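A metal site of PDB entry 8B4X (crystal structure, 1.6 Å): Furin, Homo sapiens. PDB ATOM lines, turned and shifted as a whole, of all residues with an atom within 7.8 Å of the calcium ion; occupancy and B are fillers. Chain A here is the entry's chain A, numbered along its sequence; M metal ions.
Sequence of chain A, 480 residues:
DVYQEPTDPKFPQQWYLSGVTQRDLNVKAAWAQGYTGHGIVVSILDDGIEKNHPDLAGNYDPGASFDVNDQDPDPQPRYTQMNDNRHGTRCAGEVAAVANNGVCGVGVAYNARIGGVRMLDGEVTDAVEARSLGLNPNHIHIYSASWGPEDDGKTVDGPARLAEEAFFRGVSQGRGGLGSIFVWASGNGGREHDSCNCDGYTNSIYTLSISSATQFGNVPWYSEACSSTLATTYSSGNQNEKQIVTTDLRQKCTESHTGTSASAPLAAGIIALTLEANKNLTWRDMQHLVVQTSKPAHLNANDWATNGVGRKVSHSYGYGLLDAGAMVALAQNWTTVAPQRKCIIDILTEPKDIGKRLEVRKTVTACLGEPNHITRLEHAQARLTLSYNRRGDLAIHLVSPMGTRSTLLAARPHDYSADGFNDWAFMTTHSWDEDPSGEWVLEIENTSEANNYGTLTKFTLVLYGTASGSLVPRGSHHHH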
ATOM      1  N   PRO A   6     -16.554  23.386 -19.942  1.00  0.00           N
ATOM      2  CA  PRO A   6     -15.935  24.606 -20.473  1.00  0.00           C
ATOM      3  C   PRO A   6     -16.415  24.967 -21.856  1.00  0.00           C
ATOM      4  O   PRO A   6     -16.699  24.099 -22.692  1.00  0.00           O
ATOM      5  CB  PRO A   6     -14.436  24.266 -20.483  1.00  0.00           C
ATOM      6  CG  PRO A   6     -14.294  23.294 -19.346  1.00  0.00           C
ATOM      7  CD  PRO A   6     -15.543  22.447 -19.432  1.00  0.00           C
ATOM      8  N   THR A   7     -16.439  26.274 -22.119  1.00  0.00           N
ATOM      9  CA  THR A   7     -16.839  26.851 -23.394  1.00  0.00           C
ATOM     10  C   THR A   7     -15.656  27.241 -24.268  1.00  0.00           C
ATOM     11  O   THR A   7     -15.849  27.801 -25.353  1.00  0.00           O
ATOM     12  CB  THR A   7     -17.723  28.077 -23.155  1.00  0.00           C
ATOM     13  OG1 THR A   7     -17.021  29.017 -22.335  1.00  0.00           O
ATOM     14  CG2 THR A   7     -19.002  27.676 -22.430  1.00  0.00           C
ATOM     15  N   ASP A   8     -14.436  26.968 -23.815  1.00  0.00           N
ATOM     16  CA  ASP A   8     -13.253  27.415 -24.528  1.00  0.00           C
ATOM     17  C   ASP A   8     -13.245  26.894 -25.965  1.00  0.00           C
ATOM     18  O   ASP A   8     -13.697  25.786 -26.233  1.00  0.00           O
ATOM     19  CB  ASP A   8     -12.002  26.960 -23.797  1.00  0.00           C
ATOM     20  CG  ASP A   8     -11.973  27.421 -22.362  1.00  0.00           C
ATOM     21  OD1 ASP A   8     -12.867  27.016 -21.580  1.00  0.00           O
ATOM     22  OD2 ASP A   8     -11.072  28.213 -22.023  1.00  0.00           O
ATOM     23  N   PRO A   9     -12.683  27.672 -26.898  1.00  0.00           N
ATOM     24  CA  PRO A   9     -12.832  27.339 -28.332  1.00  0.00           C
ATOM     25  C   PRO A   9     -12.197  26.019 -28.737  1.00  0.00           C
ATOM     26  O   PRO A   9     -12.695  25.374 -29.673  1.00  0.00           O
ATOM     27  CB  PRO A   9     -12.169  28.529 -29.045  1.00  0.00           C
ATOM     28  CG  PRO A   9     -11.276  29.157 -28.026  1.00  0.00           C
ATOM     29  CD  PRO A   9     -11.979  28.960 -26.704  1.00  0.00           C
ATOM     30  N   LYS A  10     -11.106  25.609 -28.101  1.00  0.00           N
ATOM     31  CA  LYS A  10     -10.476  24.345 -28.433  1.00  0.00           C
ATOM     32  C   LYS A  10     -10.824  23.223 -27.447  1.00  0.00           C
ATOM     33  O   LYS A  10     -10.272  22.128 -27.548  1.00  0.00           O
ATOM     34  CB  LYS A  10      -8.949  24.486 -28.506  1.00  0.00           C
ATOM     35  CG  LYS A  10      -8.459  25.547 -29.495  1.00  0.00           C
ATOM     36  CD  LYS A  10      -8.797  25.206 -30.932  1.00  0.00           C
ATOM     37  CE  LYS A  10      -8.357  26.318 -31.893  1.00  0.00           C
ATOM     38  N   PHE A  11     -11.733  23.471 -26.493  1.00  0.00           N
ATOM     39  CA  PHE A  11     -12.085  22.376 -25.582  1.00  0.00           C
ATOM     40  C   PHE A  11     -12.676  21.193 -26.337  1.00  0.00           C
ATOM     41  O   PHE A  11     -12.345  20.044 -25.972  1.00  0.00           O
ATOM     42  CB  PHE A  11     -13.037  22.833 -24.475  1.00  0.00           C
ATOM     43  CG  PHE A  11     -13.538  21.692 -23.621  1.00  0.00           C
ATOM     44  CD1 PHE A  11     -12.681  21.019 -22.751  1.00  0.00           C
ATOM     45  CD2 PHE A  11     -14.846  21.264 -23.705  1.00  0.00           C
ATOM     46  CE1 PHE A  11     -13.133  19.955 -21.987  1.00  0.00           C
ATOM     47  CE2 PHE A  11     -15.302  20.206 -22.948  1.00  0.00           C
ATOM     48  CZ  PHE A  11     -14.451  19.547 -22.091  1.00  0.00           C
ATOM     49  N   GLN A  14     -10.143  18.611 -27.118  1.00  0.00           N
ATOM     50  CA  GLN A  14      -9.438  17.942 -26.018  1.00  0.00           C
ATOM     51  C   GLN A  14     -10.104  16.588 -25.764  1.00  0.00           C
ATOM     52  O   GLN A  14     -10.727  16.315 -24.728  1.00  0.00           O
ATOM     53  CB  GLN A  14      -9.407  18.831 -24.791  1.00  0.00           C
ATOM     54  CG  GLN A  14      -8.656  20.117 -25.105  1.00  0.00           C
ATOM     55  CD  GLN A  14      -8.410  20.995 -23.903  1.00  0.00           C
ATOM     56  OE1 GLN A  14      -9.277  21.768 -23.506  1.00  0.00           O
ATOM     57  NE2 GLN A  14      -7.217  20.890 -23.331  1.00  0.00           N
ATOM     58  N   PRO A  54      -2.065  34.477 -22.190  1.00  0.00           N
ATOM     59  CA  PRO A  54      -3.477  34.750 -21.885  1.00  0.00           C
ATOM     60  C   PRO A  54      -4.234  33.563 -21.307  1.00  0.00           C
ATOM     61  O   PRO A  54      -5.270  33.767 -20.654  1.00  0.00           O
ATOM     62  CB  PRO A  54      -4.063  35.205 -23.234  1.00  0.00           C
ATOM     63  CG  PRO A  54      -3.015  34.944 -24.257  1.00  0.00           C
ATOM     64  CD  PRO A  54      -1.693  34.847 -23.568  1.00  0.00           C
ATOM     65  N   ASP A  55      -3.745  32.325 -21.466  1.00  0.00           N
ATOM     66  CA  ASP A  55      -4.406  31.193 -20.830  1.00  0.00           C
ATOM     67  C   ASP A  55      -3.688  30.689 -19.585  1.00  0.00           C
ATOM     68  O   ASP A  55      -4.148  29.709 -18.985  1.00  0.00           O
ATOM     69  CB  ASP A  55      -4.593  30.044 -21.839  1.00  0.00           C
ATOM     70  CG  ASP A  55      -6.027  29.487 -21.866  1.00  0.00           C
ATOM     71  OD1 ASP A  55      -6.983  30.185 -21.447  1.00  0.00           O
ATOM     72  OD2 ASP A  55      -6.199  28.327 -22.304  1.00  0.00           O
ATOM     73  N   LEU A  56      -2.595  31.326 -19.157  1.00  0.00           N
ATOM     74  CA  LEU A  56      -1.927  30.981 -17.911  1.00  0.00           C
ATOM     75  C   LEU A  56      -1.963  32.082 -16.856  1.00  0.00           C
ATOM     76  O   LEU A  56      -1.910  31.776 -15.650  1.00  0.00           O
ATOM     77  CB  LEU A  56      -0.465  30.607 -18.160  1.00  0.00           C
ATOM     78  CG  LEU A  56      -0.231  29.431 -19.109  1.00  0.00           C
ATOM     79  CD1 LEU A  56       1.266  29.225 -19.382  1.00  0.00           C
ATOM     80  CD2 LEU A  56      -0.825  28.142 -18.553  1.00  0.00           C
ATOM     81  N   ALA A  96      -3.053  23.456 -16.150  1.00  0.00           N
ATOM     82  CA  ALA A  96      -3.798  24.521 -15.511  1.00  0.00           C
ATOM     83  C   ALA A  96      -4.140  25.683 -16.434  1.00  0.00           C
ATOM     84  O   ALA A  96      -4.281  26.820 -15.961  1.00  0.00           O
ATOM     85  CB  ALA A  96      -3.020  25.079 -14.308  1.00  0.00           C
ATOM     86  N   ALA A  97      -4.281  25.443 -17.733  1.00  0.00           N
ATOM     87  CA  ALA A  97      -4.789  26.506 -18.581  1.00  0.00           C
ATOM     88  C   ALA A  97      -6.151  26.964 -18.069  1.00  0.00           C
ATOM     89  O   ALA A  97      -6.991  26.158 -17.651  1.00  0.00           O
ATOM     90  CB  ALA A  97      -4.916  26.034 -20.032  1.00  0.00           C
ATOM     91  N   VAL A  98      -6.384  28.289 -18.108  1.00  0.00           N
ATOM     92  CA  VAL A  98      -7.619  28.854 -17.586  1.00  0.00           C
ATOM     93  C   VAL A  98      -8.811  28.396 -18.412  1.00  0.00           C
ATOM     94  O   VAL A  98      -8.725  28.213 -19.633  1.00  0.00           O
ATOM     95  CB  VAL A  98      -7.517  30.397 -17.577  1.00  0.00           C
ATOM     96  CG1 VAL A  98      -8.854  31.078 -17.280  1.00  0.00           C
ATOM     97  CG2 VAL A  98      -6.439  30.826 -16.584  1.00  0.00           C
ATOM     98  N   ALA A  99      -9.944  28.226 -17.738  1.00  0.00           N
ATOM     99  CA  ALA A  99     -11.175  27.779 -18.375  1.00  0.00           C
ATOM    100  C   ALA A  99     -12.152  28.936 -18.579  1.00  0.00           C
ATOM    101  O   ALA A  99     -12.125  29.930 -17.849  1.00  0.00           O
ATOM    102  CB  ALA A  99     -11.859  26.693 -17.550  1.00  0.00           C
ATOM    103  N   ASN A 100     -13.007  28.782 -19.597  1.00  0.00           N
ATOM    104  CA  ASN A 100     -14.165  29.655 -19.817  1.00  0.00           C
ATOM    105  C   ASN A 100     -13.752  31.093 -20.073  1.00  0.00           C
ATOM    106  O   ASN A 100     -14.450  32.035 -19.680  1.00  0.00           O
ATOM    107  CB  ASN A 100     -15.136  29.568 -18.641  1.00  0.00           C
ATOM    108  CG  ASN A 100     -15.788  28.208 -18.516  1.00  0.00           C
ATOM    109  OD1 ASN A 100     -16.362  27.697 -19.478  1.00  0.00           O
ATOM    110  ND2 ASN A 100     -15.680  27.610 -17.345  1.00  0.00           N
ATOM    111  N   ASN A 101     -12.625  31.277 -20.761  1.00  0.00           N
ATOM    112  CA  ASN A 101     -12.096  32.607 -21.025  1.00  0.00           C
ATOM    113  C   ASN A 101     -11.913  32.876 -22.513  1.00  0.00           C
ATOM    114  O   ASN A 101     -11.224  33.827 -22.885  1.00  0.00           O
ATOM    115  CB  ASN A 101     -10.780  32.801 -20.278  1.00  0.00           C
ATOM    116  CG  ASN A 101      -9.668  31.944 -20.834  1.00  0.00           C
ATOM    117  OD1 ASN A 101      -9.919  30.909 -21.452  1.00  0.00           O
ATOM    118  ND2 ASN A 101      -8.429  32.370 -20.634  1.00  0.00           N
ATOM    119  N   GLY A 102     -12.515  32.055 -23.375  1.00  0.00           N
ATOM    120  CA  GLY A 102     -12.460  32.317 -24.803  1.00  0.00           C
ATOM    121  C   GLY A 102     -11.114  32.085 -25.451  1.00  0.00           C
ATOM    122  O   GLY A 102     -10.933  32.469 -26.618  1.00  0.00           O
ATOM    123  N   VAL A 103     -10.168  31.452 -24.756  1.00  0.00           N
ATOM    124  CA  VAL A 103      -8.810  31.272 -25.240  1.00  0.00           C
ATOM    125  C   VAL A 103      -8.451  29.784 -25.196  1.00  0.00           C
ATOM    126  O   VAL A 103      -8.640  29.129 -24.164  1.00  0.00           O
ATOM    127  CB  VAL A 103      -7.790  32.072 -24.398  1.00  0.00           C
ATOM    128  CG1 VAL A 103      -6.363  31.786 -24.869  1.00  0.00           C
ATOM    129  CG2 VAL A 103      -8.106  33.558 -24.404  1.00  0.00           C
ATOM    130  N   CYS A 104      -7.983  29.255 -26.333  1.00  0.00           N
ATOM    131  CA  CYS A 104      -7.392  27.901 -26.444  1.00  0.00           C
ATOM    132  C   CYS A 104      -8.300  26.896 -25.739  1.00  0.00           C
ATOM    133  O   CYS A 104      -9.505  26.865 -26.016  1.00  0.00           O
ATOM    134  CB  CYS A 104      -5.954  27.967 -25.935  1.00  0.00           C
ATOM    135  SG  CYS A 104      -4.871  26.586 -26.411  1.00  0.00           S
ATOM    136  N   GLY A 105      -7.761  26.036 -24.879  1.00  0.00           N
ATOM    137  CA  GLY A 105      -8.555  24.994 -24.229  1.00  0.00           C
ATOM    138  C   GLY A 105      -8.527  25.170 -22.738  1.00  0.00           C
ATOM    139  O   GLY A 105      -8.519  26.304 -22.259  1.00  0.00           O
ATOM    140  N   VAL A 106      -8.503  24.070 -21.975  1.00  0.00           N
ATOM    141  CA  VAL A 106      -8.483  24.131 -20.522  1.00  0.00           C
ATOM    142  C   VAL A 106      -7.436  23.175 -19.970  1.00  0.00           C
ATOM    143  O   VAL A 106      -7.120  22.144 -20.587  1.00  0.00           O
ATOM    144  CB  VAL A 106      -9.859  23.797 -19.881  1.00  0.00           C
ATOM    145  CG1 VAL A 106     -10.943  24.670 -20.484  1.00  0.00           C
ATOM    146  CG2 VAL A 106     -10.175  22.313 -20.020  1.00  0.00           C
ATOM    147  N   GLY A 107      -6.918  23.488 -18.785  1.00  0.00           N
ATOM    148  CA  GLY A 107      -6.131  22.529 -18.052  1.00  0.00           C
ATOM    149  C   GLY A 107      -6.983  21.452 -17.399  1.00  0.00           C
ATOM    150  O   GLY A 107      -8.186  21.608 -17.211  1.00  0.00           O
ATOM    151  N   TYR A 110      -8.072  23.292 -14.030  1.00  0.00           N
ATOM    152  CA  TYR A 110      -8.113  24.632 -14.577  1.00  0.00           C
ATOM    153  C   TYR A 110      -8.331  25.725 -13.541  1.00  0.00           C
ATOM    154  O   TYR A 110      -8.277  26.907 -13.903  1.00  0.00           O
ATOM    155  CB  TYR A 110      -9.175  24.696 -15.674  1.00  0.00           C
ATOM    156  CG  TYR A 110     -10.605  24.311 -15.340  1.00  0.00           C
ATOM    157  CD1 TYR A 110     -11.400  25.107 -14.521  1.00  0.00           C
ATOM    158  CD2 TYR A 110     -11.192  23.200 -15.951  1.00  0.00           C
ATOM    159  CE1 TYR A 110     -12.728  24.778 -14.278  1.00  0.00           C
ATOM    160  CE2 TYR A 110     -12.523  22.877 -15.715  1.00  0.00           C
ATOM    161  CZ  TYR A 110     -13.279  23.664 -14.878  1.00  0.00           C
ATOM    162  OH  TYR A 110     -14.601  23.335 -14.652  1.00  0.00           O
ATOM    163  N   THR A 247      -1.200  25.540 -24.265  1.00  0.00           N
ATOM    164  CA  THR A 247      -0.631  26.869 -24.430  1.00  0.00           C
ATOM    165  C   THR A 247       0.752  26.785 -25.036  1.00  0.00           C
ATOM    166  O   THR A 247       1.571  25.950 -24.636  1.00  0.00           O
ATOM    167  CB  THR A 247      -0.553  27.549 -23.062  1.00  0.00           C
ATOM    168  OG1 THR A 247       0.047  26.647 -22.122  1.00  0.00           O
ATOM    169  CG2 THR A 247      -1.931  27.926 -22.564  1.00  0.00           C
HETATM  170 CA    CA M   1      -8.770  28.660 -21.880  1.00  0.00          CA
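The calcium ion is bound by the backbone carbonyl oxygen (O) of Val 98, the backbone carbonyl oxygen (O) of Val 103, the side-chain carboxylate (OD2) of Asp 8, the side-chain carboxylate (OD1) of Asp 55, the backbone carbonyl oxygen (O) of Gly 105, the side-chain amide oxygen (OD1) of Asn 101 and the side-chain carboxylate (OD2) of Asp 55. The calcium ion has seven donor atoms within binding distance.
The side-chain carboxylate of Asp 8 lies within hydrogen-bond range of the backbone NH of Asn 100 (2.7 Å). The side-chain amide nitrogen (ND2) of Asn 101 is in hydrogen-bond range of the backbone carbonyl oxygen (O) of Pro 54.
Within 4 Å of the calcium ion: Asp 8, Asp 55, Val 98, Asn 101, Val 103 and Gly 105. The nearest printed residue that does not touch the calcium ion is Cys 104 (4.3 Å).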
